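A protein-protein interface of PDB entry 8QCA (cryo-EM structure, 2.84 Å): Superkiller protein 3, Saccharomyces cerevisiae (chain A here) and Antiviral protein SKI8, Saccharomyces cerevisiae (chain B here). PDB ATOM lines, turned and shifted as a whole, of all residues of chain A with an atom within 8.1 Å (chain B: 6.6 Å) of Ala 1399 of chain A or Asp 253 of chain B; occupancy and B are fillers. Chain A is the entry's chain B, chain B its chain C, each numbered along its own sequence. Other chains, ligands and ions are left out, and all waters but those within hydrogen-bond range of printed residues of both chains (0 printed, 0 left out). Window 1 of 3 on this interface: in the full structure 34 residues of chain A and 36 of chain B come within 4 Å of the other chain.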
ATOM      1  N   LYS A1396       0.118   5.962  -4.224  1.00  0.00           N
ATOM      2  CA  LYS A1396       0.790   6.815  -3.256  1.00  0.00           C
ATOM      3  C   LYS A1396       1.323   5.956  -2.116  1.00  0.00           C
ATOM      4  O   LYS A1396       0.543   5.352  -1.371  1.00  0.00           O
ATOM      5  CB  LYS A1396      -0.168   7.885  -2.736  1.00  0.00           C
ATOM      6  CG  LYS A1396      -0.715   8.783  -3.831  1.00  0.00           C
ATOM      7  CD  LYS A1396      -1.739   9.762  -3.295  1.00  0.00           C
ATOM      8  CE  LYS A1396      -1.653  11.089  -4.024  1.00  0.00           C
ATOM      9  NZ  LYS A1396      -2.068  10.966  -5.447  1.00  0.00           N
ATOM     10  N   VAL A1397       2.646   5.906  -1.981  1.00  0.00           N
ATOM     11  CA  VAL A1397       3.314   5.038  -1.020  1.00  0.00           C
ATOM     12  C   VAL A1397       4.250   5.882  -0.164  1.00  0.00           C
ATOM     13  O   VAL A1397       4.863   6.838  -0.651  1.00  0.00           O
ATOM     14  CB  VAL A1397       4.074   3.893  -1.730  1.00  0.00           C
ATOM     15  CG1 VAL A1397       5.348   4.398  -2.389  1.00  0.00           C
ATOM     16  CG2 VAL A1397       4.378   2.771  -0.762  1.00  0.00           C
ATOM     17  N   THR A1398       4.340   5.542   1.119  1.00  0.00           N
ATOM     18  CA  THR A1398       5.161   6.299   2.050  1.00  0.00           C
ATOM     19  C   THR A1398       6.617   5.841   1.984  1.00  0.00           C
ATOM     20  O   THR A1398       6.962   4.852   1.334  1.00  0.00           O
ATOM     21  CB  THR A1398       4.626   6.160   3.475  1.00  0.00           C
ATOM     22  OG1 THR A1398       5.005   4.888   4.011  1.00  0.00           O
ATOM     23  CG2 THR A1398       3.113   6.278   3.489  1.00  0.00           C
ATOM     24  N   ALA A1399       7.483   6.590   2.674  1.00  0.00           N
ATOM     25  CA  ALA A1399       8.911   6.289   2.647  1.00  0.00           C
ATOM     26  C   ALA A1399       9.219   4.968   3.341  1.00  0.00           C
ATOM     27  O   ALA A1399      10.063   4.198   2.868  1.00  0.00           O
ATOM     28  CB  ALA A1399       9.700   7.430   3.286  1.00  0.00           C
ATOM     29  N   GLU A1400       8.552   4.689   4.463  1.00  0.00           N
ATOM     30  CA  GLU A1400       8.785   3.430   5.164  1.00  0.00           C
ATOM     31  C   GLU A1400       8.358   2.236   4.319  1.00  0.00           C
ATOM     32  O   GLU A1400       9.087   1.241   4.222  1.00  0.00           O
ATOM     33  CB  GLU A1400       8.044   3.429   6.501  1.00  0.00           C
ATOM     34  CG  GLU A1400       8.827   4.039   7.652  1.00  0.00           C
ATOM     35  CD  GLU A1400       8.512   5.509   7.857  1.00  0.00           C
ATOM     36  OE1 GLU A1400       8.238   6.207   6.857  1.00  0.00           O
ATOM     37  OE2 GLU A1400       8.534   5.967   9.019  1.00  0.00           O
ATOM     38  N   GLU A1401       7.183   2.320   3.691  1.00  0.00           N
ATOM     39  CA  GLU A1401       6.708   1.218   2.860  1.00  0.00           C
ATOM     40  C   GLU A1401       7.590   1.024   1.633  1.00  0.00           C
ATOM     41  O   GLU A1401       7.898  -0.113   1.257  1.00  0.00           O
ATOM     42  CB  GLU A1401       5.256   1.460   2.451  1.00  0.00           C
ATOM     43  CG  GLU A1401       4.320   1.710   3.622  1.00  0.00           C
ATOM     44  CD  GLU A1401       2.903   2.030   3.185  1.00  0.00           C
ATOM     45  OE1 GLU A1401       2.718   2.475   2.033  1.00  0.00           O
ATOM     46  OE2 GLU A1401       1.973   1.836   3.995  1.00  0.00           O
ATOM     47  N   MET A1402       8.005   2.118   0.992  1.00  0.00           N
ATOM     48  CA  MET A1402       8.878   2.000  -0.171  1.00  0.00           C
ATOM     49  C   MET A1402      10.224   1.400   0.217  1.00  0.00           C
ATOM     50  O   MET A1402      10.780   0.569  -0.514  1.00  0.00           O
ATOM     51  CB  MET A1402       9.067   3.368  -0.824  1.00  0.00           C
ATOM     52  CG  MET A1402       9.499   3.308  -2.279  1.00  0.00           C
ATOM     53  SD  MET A1402       8.347   2.324  -3.260  1.00  0.00           S
ATOM     54  CE  MET A1402       9.413   1.726  -4.562  1.00  0.00           C
ATOM     55  N   SER A1403      10.765   1.813   1.368  1.00  0.00           N
ATOM     56  CA  SER A1403      12.013   1.240   1.857  1.00  0.00           C
ATOM     57  C   SER A1403      11.856  -0.245   2.152  1.00  0.00           C
ATOM     58  O   SER A1403      12.774  -1.035   1.905  1.00  0.00           O
ATOM     59  CB  SER A1403      12.476   1.989   3.105  1.00  0.00           C
ATOM     60  OG  SER A1403      13.402   1.218   3.848  1.00  0.00           O
ATOM     61  N   LYS A1404      10.701  -0.641   2.689  1.00  0.00           N
ATOM     62  CA  LYS A1404      10.429  -2.060   2.891  1.00  0.00           C
ATOM     63  C   LYS A1404      10.393  -2.806   1.563  1.00  0.00           C
ATOM     64  O   LYS A1404      10.856  -3.949   1.468  1.00  0.00           O
ATOM     65  CB  LYS A1404       9.109  -2.232   3.643  1.00  0.00           C
ATOM     66  CG  LYS A1404       8.772  -3.666   3.999  1.00  0.00           C
ATOM     67  CD  LYS A1404       7.551  -3.730   4.899  1.00  0.00           C
ATOM     68  CE  LYS A1404       6.661  -4.904   4.536  1.00  0.00           C
ATOM     69  NZ  LYS A1404       6.230  -4.849   3.112  1.00  0.00           N
ATOM     70  N   LEU A1405       9.835  -2.178   0.526  1.00  0.00           N
ATOM     71  CA  LEU A1405       9.796  -2.809  -0.791  1.00  0.00           C
ATOM     72  C   LEU A1405      11.195  -2.981  -1.374  1.00  0.00           C
ATOM     73  O   LEU A1405      11.497  -4.018  -1.977  1.00  0.00           O
ATOM     74  CB  LEU A1405       8.917  -1.995  -1.739  1.00  0.00           C
ATOM     75  CG  LEU A1405       7.438  -1.879  -1.371  1.00  0.00           C
ATOM     76  CD1 LEU A1405       6.721  -0.933  -2.317  1.00  0.00           C
ATOM     77  CD2 LEU A1405       6.783  -3.244  -1.379  1.00  0.00           C
ATOM     78  N   TYR A1406      12.059  -1.971  -1.224  1.00  0.00           N
ATOM     79  CA  TYR A1406      13.432  -2.092  -1.716  1.00  0.00           C
ATOM     80  C   TYR A1406      14.188  -3.224  -1.034  1.00  0.00           C
ATOM     81  O   TYR A1406      14.878  -4.005  -1.700  1.00  0.00           O
ATOM     82  CB  TYR A1406      14.184  -0.772  -1.537  1.00  0.00           C
ATOM     83  CG  TYR A1406      13.790   0.303  -2.518  1.00  0.00           C
ATOM     84  CD1 TYR A1406      13.116  -0.015  -3.685  1.00  0.00           C
ATOM     85  CD2 TYR A1406      14.091   1.634  -2.279  1.00  0.00           C
ATOM     86  CE1 TYR A1406      12.763   0.959  -4.593  1.00  0.00           C
ATOM     87  CE2 TYR A1406      13.734   2.617  -3.178  1.00  0.00           C
ATOM     88  CZ  TYR A1406      13.068   2.273  -4.333  1.00  0.00           C
ATOM     89  OH  TYR A1406      12.710   3.248  -5.233  1.00  0.00           O
ATOM     90  N   ARG A1417      19.855   1.096  -0.770  1.00  0.00           N
ATOM     91  CA  ARG A1417      18.888   2.131  -1.126  1.00  0.00           C
ATOM     92  C   ARG A1417      17.799   2.262  -0.062  1.00  0.00           C
ATOM     93  O   ARG A1417      17.465   3.373   0.378  1.00  0.00           O
ATOM     94  CB  ARG A1417      18.281   1.797  -2.487  1.00  0.00           C
ATOM     95  CG  ARG A1417      17.520   2.911  -3.160  1.00  0.00           C
ATOM     96  CD  ARG A1417      17.024   2.427  -4.505  1.00  0.00           C
ATOM     97  NE  ARG A1417      18.134   1.994  -5.345  1.00  0.00           N
ATOM     98  CZ  ARG A1417      18.003   1.272  -6.448  1.00  0.00           C
ATOM     99  NH1 ARG A1417      16.817   0.884  -6.885  1.00  0.00           N
ATOM    100  NH2 ARG A1417      19.093   0.925  -7.129  1.00  0.00           N
ATOM    101  N   GLY A1418      17.245   1.130   0.375  1.00  0.00           N
ATOM    102  CA  GLY A1418      16.181   1.158   1.361  1.00  0.00           C
ATOM    103  C   GLY A1418      16.647   1.569   2.741  1.00  0.00           C
ATOM    104  O   GLY A1418      15.865   2.115   3.524  1.00  0.00           O
ATOM    105  N   LEU A1421      16.930   5.380   2.509  1.00  0.00           N
ATOM    106  CA  LEU A1421      15.631   6.045   2.596  1.00  0.00           C
ATOM    107  C   LEU A1421      15.157   6.162   4.042  1.00  0.00           C
ATOM    108  O   LEU A1421      14.761   7.244   4.488  1.00  0.00           O
ATOM    109  CB  LEU A1421      14.594   5.303   1.756  1.00  0.00           C
ATOM    110  CG  LEU A1421      14.464   5.734   0.296  1.00  0.00           C
ATOM    111  CD1 LEU A1421      13.660   4.713  -0.475  1.00  0.00           C
ATOM    112  CD2 LEU A1421      13.818   7.105   0.201  1.00  0.00           C
ATOM    113  N   CYS A1422      15.190   5.061   4.789  1.00  0.00           N
ATOM    114  CA  CYS A1422      14.690   5.017   6.164  1.00  0.00           C
ATOM    115  C   CYS A1422      15.764   4.408   7.055  1.00  0.00           C
ATOM    116  O   CYS A1422      15.734   3.208   7.355  1.00  0.00           O
ATOM    117  CB  CYS A1422      13.381   4.229   6.245  1.00  0.00           C
ATOM    118  SG  CYS A1422      12.671   4.095   7.897  1.00  0.00           S
ATOM    119  N   TRP A1424      16.237   4.528  10.182  1.00  0.00           N
ATOM    120  CA  TRP A1424      15.758   4.031  11.464  1.00  0.00           C
ATOM    121  C   TRP A1424      14.978   2.730  11.340  1.00  0.00           C
ATOM    122  O   TRP A1424      14.528   2.196  12.359  1.00  0.00           O
ATOM    123  CB  TRP A1424      14.893   5.085  12.163  1.00  0.00           C
ATOM    124  CG  TRP A1424      13.831   5.674  11.299  1.00  0.00           C
ATOM    125  CD1 TRP A1424      12.537   5.260  11.194  1.00  0.00           C
ATOM    126  CD2 TRP A1424      13.965   6.795  10.421  1.00  0.00           C
ATOM    127  NE1 TRP A1424      11.858   6.050  10.300  1.00  0.00           N
ATOM    128  CE2 TRP A1424      12.715   7.001   9.811  1.00  0.00           C
ATOM    129  CE3 TRP A1424      15.025   7.642  10.088  1.00  0.00           C
ATOM    130  CZ2 TRP A1424      12.494   8.017   8.889  1.00  0.00           C
ATOM    131  CZ3 TRP A1424      14.803   8.650   9.173  1.00  0.00           C
ATOM    132  CH2 TRP A1424      13.548   8.829   8.583  1.00  0.00           C
ATOM    133  N   ASN A1425      14.800   2.213  10.128  1.00  0.00           N
ATOM    134  CA  ASN A1425      14.133   0.932   9.955  1.00  0.00           C
ATOM    135  C   ASN A1425      15.002  -0.193  10.503  1.00  0.00           C
ATOM    136  O   ASN A1425      16.218  -0.221  10.296  1.00  0.00           O
ATOM    137  CB  ASN A1425      13.825   0.691   8.478  1.00  0.00           C
ATOM    138  CG  ASN A1425      12.829  -0.430   8.265  1.00  0.00           C
ATOM    139  OD1 ASN A1425      12.025  -0.739   9.146  1.00  0.00           O
ATOM    140  ND2 ASN A1425      12.870  -1.042   7.087  1.00  0.00           N
ATOM    141  N   SER B 225       7.506  21.098  12.152  1.00  0.00           N
ATOM    142  CA  SER B 225       7.081  21.357  10.784  1.00  0.00           C
ATOM    143  C   SER B 225       6.028  20.372  10.287  1.00  0.00           C
ATOM    144  O   SER B 225       5.678  20.406   9.104  1.00  0.00           O
ATOM    145  CB  SER B 225       8.290  21.341   9.848  1.00  0.00           C
ATOM    146  OG  SER B 225       8.885  20.056   9.805  1.00  0.00           O
ATOM    147  N   GLN B 226       5.516  19.504  11.156  1.00  0.00           N
ATOM    148  CA  GLN B 226       4.542  18.509  10.730  1.00  0.00           C
ATOM    149  C   GLN B 226       3.229  19.173  10.337  1.00  0.00           C
ATOM    150  O   GLN B 226       2.705  20.019  11.068  1.00  0.00           O
ATOM    151  CB  GLN B 226       4.299  17.493  11.843  1.00  0.00           C
ATOM    152  CG  GLN B 226       5.521  16.688  12.234  1.00  0.00           C
ATOM    153  CD  GLN B 226       6.084  17.104  13.575  1.00  0.00           C
ATOM    154  OE1 GLN B 226       6.301  18.286  13.828  1.00  0.00           O
ATOM    155  NE2 GLN B 226       6.321  16.131  14.446  1.00  0.00           N
ATOM    156  N   HIS B 227       2.697  18.786   9.176  1.00  0.00           N
ATOM    157  CA  HIS B 227       1.374  19.256   8.777  1.00  0.00           C
ATOM    158  C   HIS B 227       0.301  18.738   9.727  1.00  0.00           C
ATOM    159  O   HIS B 227      -0.611  19.478  10.109  1.00  0.00           O
ATOM    160  CB  HIS B 227       1.073  18.825   7.342  1.00  0.00           C
ATOM    161  CG  HIS B 227       1.792  19.628   6.304  1.00  0.00           C
ATOM    162  ND1 HIS B 227       1.438  19.609   4.972  1.00  0.00           N
ATOM    163  CD2 HIS B 227       2.847  20.470   6.400  1.00  0.00           C
ATOM    164  CE1 HIS B 227       2.242  20.407   4.293  1.00  0.00           C
ATOM    165  NE2 HIS B 227       3.107  20.941   5.137  1.00  0.00           N
ATOM    166  N   SER B 233       4.647   9.782   9.592  1.00  0.00           N
ATOM    167  CA  SER B 233       5.428  10.208   8.436  1.00  0.00           C
ATOM    168  C   SER B 233       6.105  11.545   8.712  1.00  0.00           C
ATOM    169  O   SER B 233       6.240  11.952   9.870  1.00  0.00           O
ATOM    170  CB  SER B 233       4.541  10.306   7.193  1.00  0.00           C
ATOM    171  N   ASN B 234       6.561  12.211   7.650  1.00  0.00           N
ATOM    172  CA  ASN B 234       7.111  13.561   7.719  1.00  0.00           C
ATOM    173  C   ASN B 234       8.420  13.647   8.493  1.00  0.00           C
ATOM    174  O   ASN B 234       8.523  14.404   9.464  1.00  0.00           O
ATOM    175  CB  ASN B 234       6.088  14.523   8.333  1.00  0.00           C
ATOM    176  N   SER B 235       9.423  12.890   8.068  1.00  0.00           N
ATOM    177  CA  SER B 235      10.777  13.056   8.568  1.00  0.00           C
ATOM    178  C   SER B 235      11.497  14.150   7.784  1.00  0.00           C
ATOM    179  O   SER B 235      11.077  14.548   6.697  1.00  0.00           O
ATOM    180  CB  SER B 235      11.555  11.743   8.473  1.00  0.00           C
ATOM    181  OG  SER B 235      11.635  11.292   7.134  1.00  0.00           O
ATOM    182  N   ILE B 236      12.598  14.632   8.353  1.00  0.00           N
ATOM    183  CA  ILE B 236      13.394  15.696   7.751  1.00  0.00           C
ATOM    184  C   ILE B 236      14.529  15.069   6.958  1.00  0.00           C
ATOM    185  O   ILE B 236      15.268  14.223   7.477  1.00  0.00           O
ATOM    186  CB  ILE B 236      13.938  16.657   8.821  1.00  0.00           C
ATOM    187  CG1 ILE B 236      12.803  17.479   9.419  1.00  0.00           C
ATOM    188  CG2 ILE B 236      14.999  17.572   8.232  1.00  0.00           C
ATOM    189  CD1 ILE B 236      12.959  17.710  10.886  1.00  0.00           C
ATOM    190  N   ARG B 237      14.671  15.485   5.700  1.00  0.00           N
ATOM    191  CA  ARG B 237      15.705  14.953   4.823  1.00  0.00           C
ATOM    192  C   ARG B 237      16.885  15.892   4.635  1.00  0.00           C
ATOM    193  O   ARG B 237      18.015  15.419   4.477  1.00  0.00           O
ATOM    194  CB  ARG B 237      15.112  14.617   3.450  1.00  0.00           C
ATOM    195  CG  ARG B 237      13.913  13.695   3.513  1.00  0.00           C
ATOM    196  CD  ARG B 237      14.027  12.576   2.501  1.00  0.00           C
ATOM    197  NE  ARG B 237      13.057  11.521   2.757  1.00  0.00           N
ATOM    198  CZ  ARG B 237      13.360  10.329   3.254  1.00  0.00           C
ATOM    199  NH1 ARG B 237      14.606   9.999   3.547  1.00  0.00           N
ATOM    200  NH2 ARG B 237      12.386   9.448   3.462  1.00  0.00           N
ATOM    201  N   ALA B 251      13.522  20.584   4.279  1.00  0.00           N
ATOM    202  CA  ALA B 251      12.894  19.619   3.387  1.00  0.00           C
ATOM    203  C   ALA B 251      12.362  18.469   4.230  1.00  0.00           C
ATOM    204  O   ALA B 251      13.133  17.794   4.919  1.00  0.00           O
ATOM    205  CB  ALA B 251      13.880  19.110   2.338  1.00  0.00           C
ATOM    206  N   HIS B 252      11.052  18.250   4.174  1.00  0.00           N
ATOM    207  CA  HIS B 252      10.411  17.232   4.990  1.00  0.00           C
ATOM    208  C   HIS B 252       9.374  16.493   4.159  1.00  0.00           C
ATOM    209  O   HIS B 252       8.845  17.016   3.175  1.00  0.00           O
ATOM    210  CB  HIS B 252       9.762  17.837   6.243  1.00  0.00           C
ATOM    211  CG  HIS B 252       8.945  19.063   5.974  1.00  0.00           C
ATOM    212  ND1 HIS B 252       7.568  19.060   6.006  1.00  0.00           N
ATOM    213  CD2 HIS B 252       9.313  20.332   5.679  1.00  0.00           C
ATOM    214  CE1 HIS B 252       7.122  20.273   5.734  1.00  0.00           C
ATOM    215  NE2 HIS B 252       8.160  21.064   5.533  1.00  0.00           N
ATOM    216  N   ASP B 253       9.093  15.260   4.567  1.00  0.00           N
ATOM    217  CA  ASP B 253       8.124  14.426   3.878  1.00  0.00           C
ATOM    218  C   ASP B 253       6.705  14.800   4.290  1.00  0.00           C
ATOM    219  O   ASP B 253       6.474  15.438   5.317  1.00  0.00           O
ATOM    220  CB  ASP B 253       8.374  12.949   4.179  1.00  0.00           C
ATOM    221  CG  ASP B 253       9.710  12.470   3.665  1.00  0.00           C
ATOM    222  OD1 ASP B 253      10.552  13.322   3.318  1.00  0.00           O
ATOM    223  OD2 ASP B 253       9.923  11.242   3.612  1.00  0.00           O
ATOM    224  N   SER B 254       5.747  14.421   3.446  1.00  0.00           N
ATOM    225  CA  SER B 254       4.334  14.480   3.824  1.00  0.00           C
ATOM    226  C   SER B 254       3.639  13.302   3.141  1.00  0.00           C
ATOM    227  O   SER B 254       3.191  13.421   2.001  1.00  0.00           O
ATOM    228  CB  SER B 254       3.707  15.810   3.434  1.00  0.00           C
ATOM    229  OG  SER B 254       2.419  15.953   4.003  1.00  0.00           O
ATOM    230  N   ASN B 255       3.604  12.163   3.843  1.00  0.00           N
ATOM    231  CA  ASN B 255       2.876  10.945   3.477  1.00  0.00           C
ATOM    232  C   ASN B 255       2.821  10.705   1.969  1.00  0.00           C
ATOM    233  O   ASN B 255       1.736  10.664   1.379  1.00  0.00           O
ATOM    234  CB  ASN B 255       1.475  10.913   4.130  1.00  0.00           C
ATOM    235  CG  ASN B 255       0.540  12.032   3.676  1.00  0.00           C
ATOM    236  OD1 ASN B 255       0.830  12.801   2.767  1.00  0.00           O
ATOM    237  ND2 ASN B 255      -0.608  12.118   4.336  1.00  0.00           N
ATOM    238  N   SER B 256       3.997  10.535   1.355  1.00  0.00           N
ATOM    239  CA  SER B 256       4.273  10.351  -0.085  1.00  0.00           C
ATOM    240  C   SER B 256       4.370  11.653  -0.871  1.00  0.00           C
ATOM    241  O   SER B 256       4.400  11.604  -2.105  1.00  0.00           O
ATOM    242  CB  SER B 256       3.246   9.463  -0.798  1.00  0.00           C
ATOM    243  OG  SER B 256       1.970  10.077  -0.840  1.00  0.00           O
ATOM    244  N   PHE B 257       4.435  12.807  -0.215  1.00  0.00           N
ATOM    245  CA  PHE B 257       4.667  14.071  -0.895  1.00  0.00           C
ATOM    246  C   PHE B 257       5.934  14.723  -0.355  1.00  0.00           C
ATOM    247  O   PHE B 257       6.446  14.355   0.704  1.00  0.00           O
ATOM    248  CB  PHE B 257       3.477  15.022  -0.730  1.00  0.00           C
ATOM    249  CG  PHE B 257       2.295  14.673  -1.588  1.00  0.00           C
ATOM    250  CD1 PHE B 257       2.289  14.977  -2.938  1.00  0.00           C
ATOM    251  CD2 PHE B 257       1.187  14.048  -1.043  1.00  0.00           C
ATOM    252  CE1 PHE B 257       1.204  14.661  -3.729  1.00  0.00           C
ATOM    253  CE2 PHE B 257       0.100  13.730  -1.829  1.00  0.00           C
ATOM    254  CZ  PHE B 257       0.108  14.038  -3.173  1.00  0.00           C
ATOM    255  N   GLY B 258       6.437  15.700  -1.103  1.00  0.00           N
ATOM    256  CA  GLY B 258       7.623  16.429  -0.698  1.00  0.00           C
ATOM    257  C   GLY B 258       7.336  17.891  -0.434  1.00  0.00           C
ATOM    258  O   GLY B 258       6.702  18.560  -1.253  1.00  0.00           O
ATOM    259  N   CYS B 259       7.802  18.403   0.702  1.00  0.00           N
ATOM    260  CA  CYS B 259       7.477  19.753   1.136  1.00  0.00           C
ATOM    261  C   CYS B 259       8.746  20.506   1.507  1.00  0.00           C
ATOM    262  O   CYS B 259       9.729  19.915   1.956  1.00  0.00           O
ATOM    263  CB  CYS B 259       6.519  19.732   2.333  1.00  0.00           C
ATOM    264  SG  CYS B 259       4.971  18.859   2.032  1.00  0.00           S
ATOM    265  N   SER B 292       7.085  13.257  -5.551  1.00  0.00           N
ATOM    266  CA  SER B 292       7.468  12.105  -4.745  1.00  0.00           C
ATOM    267  C   SER B 292       8.050  12.499  -3.393  1.00  0.00           C
ATOM    268  O   SER B 292       7.420  12.262  -2.361  1.00  0.00           O
ATOM    269  CB  SER B 292       8.472  11.240  -5.507  1.00  0.00           C
ATOM    270  OG  SER B 292       8.693  10.012  -4.840  1.00  0.00           O
ATOM    271  N   TRP B 293       9.211  13.154  -3.396  1.00  0.00           N
ATOM    272  CA  TRP B 293       9.968  13.513  -2.199  1.00  0.00           C
ATOM    273  C   TRP B 293      11.065  14.485  -2.599  1.00  0.00           C
ATOM    274  O   TRP B 293      11.520  14.482  -3.745  1.00  0.00           O
ATOM    275  CB  TRP B 293      10.608  12.298  -1.506  1.00  0.00           C
ATOM    276  CG  TRP B 293       9.665  11.349  -0.849  1.00  0.00           C
ATOM    277  CD1 TRP B 293       8.732  11.641   0.102  1.00  0.00           C
ATOM    278  CD2 TRP B 293       9.557   9.944  -1.098  1.00  0.00           C
ATOM    279  NE1 TRP B 293       8.049  10.505   0.457  1.00  0.00           N
ATOM    280  CE2 TRP B 293       8.537   9.449  -0.266  1.00  0.00           C
ATOM    281  CE3 TRP B 293      10.224   9.056  -1.947  1.00  0.00           C
ATOM    282  CZ2 TRP B 293       8.169   8.108  -0.257  1.00  0.00           C
ATOM    283  CZ3 TRP B 293       9.858   7.725  -1.935  1.00  0.00           C
ATOM    284  CH2 TRP B 293       8.840   7.264  -1.096  1.00  0.00           C
ATOM    285  N   VAL B 294      11.491  15.301  -1.642  1.00  0.00           N
ATOM    286  CA  VAL B 294      12.638  16.183  -1.812  1.00  0.00           C
ATOM    287  C   VAL B 294      13.810  15.566  -1.063  1.00  0.00           C
ATOM    288  O   VAL B 294      13.741  15.366   0.156  1.00  0.00           O
ATOM    289  CB  VAL B 294      12.337  17.603  -1.309  1.00  0.00           C
ATOM    290  CG1 VAL B 294      13.540  18.504  -1.520  1.00  0.00           C
ATOM    291  CG2 VAL B 294      11.118  18.163  -2.015  1.00  0.00           C
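Printed residues of chain B within 4 Å of Lys 1396 of chain A: Ser 256 and Phe 257.
Glu 1401 of chain A touches none of the printed residues of chain B.
Of the printed residues of chain B, Leu 1421 of chain A touches Arg 237 (2.9 Å).
Of the printed residues of chain B, Trp 1424 of chain A touches Ser 235.
Asp 253 of chain B touches just one residue of chain A: Ala 1399 (3.8 Å).
Of the printed residues of chain A, Trp 293 of chain B touches Val 1397 (3.6 Å), Thr 1398 (3.5 Å), Ala 1399 (3.4 Å) and Met 1402 (3.9 Å).
The nearest printed residue of chain A that does not touch Phe 257 of chain B is Val 1397 of chain A (6.0 Å).
Printed residues of chain B that touch a printed residue of chain A: Ser 235, Arg 237, Asp 253, Ser 256, Phe 257 and Trp 293.
Hydrophobic or aromatic side chains of chain B within 4 Å of the printed part of chain A: Phe 257 and Trp 293.
Among the printed residues, no Asp or Glu carboxylate lies within 4 Å of a Lys or Arg side-chain nitrogen of the other chain.
Among the printed residues, pairs that only touch across the chains: Val 1397 of chain A with Ser 256 of chain B (3.1 Å), Ala 1399 of chain A with Arg 237 of chain B (3.4 Å), Ala 1399 of chain A with Trp 293 of chain B (3.4 Å), Trp 1424 of chain A with Ser 235 of chain B (3.4 Å), Lys 1396 of chain A with Phe 257 of chain B (3.5 Å), Thr 1398 of chain A with Trp 293 of chain B (3.5 Å), Val 1397 of chain A with Trp 293 of chain B (3.6 Å), Lys 1396 of chain A with Ser 256 of chain B (3.6 Å), Ala 1399 of chain A with Asp 253 of chain B (3.8 Å) and Met 1402 of chain A with Trp 293 of chain B (3.9 Å).
The side-chain hydroxyl (OG1) of Thr 1398 of chain A sits close to the backbone NH (N) of Glu 1401 of chain A (3.4 Å).
The indole nitrogen (NE1) of Trp 1424 of chain A sits at hydrogen-bond distance from the side-chain sulfur (SG) of Cys 1422 of chain A, 3.2 Å away.
O of Ser 235 of chain B lies within hydrogen-bond range of N of Asp 253 of chain B (3.0 Å).
The backbone carbonyl oxygen of Ala 251 of chain B sits at hydrogen-bond distance from the backbone NH of Arg 237 of chain B (2.9 Å).
The guanidinium group of Arg 237 of chain B is in salt-bridge range of the side-chain carboxylate of Asp 253 of chain B (3.1 Å).
The backbone carbonyl oxygen of Leu 1421 of chain A is in hydrogen-bond range of the guanidinium group of Arg 237 of chain B, 2.9 Å away.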
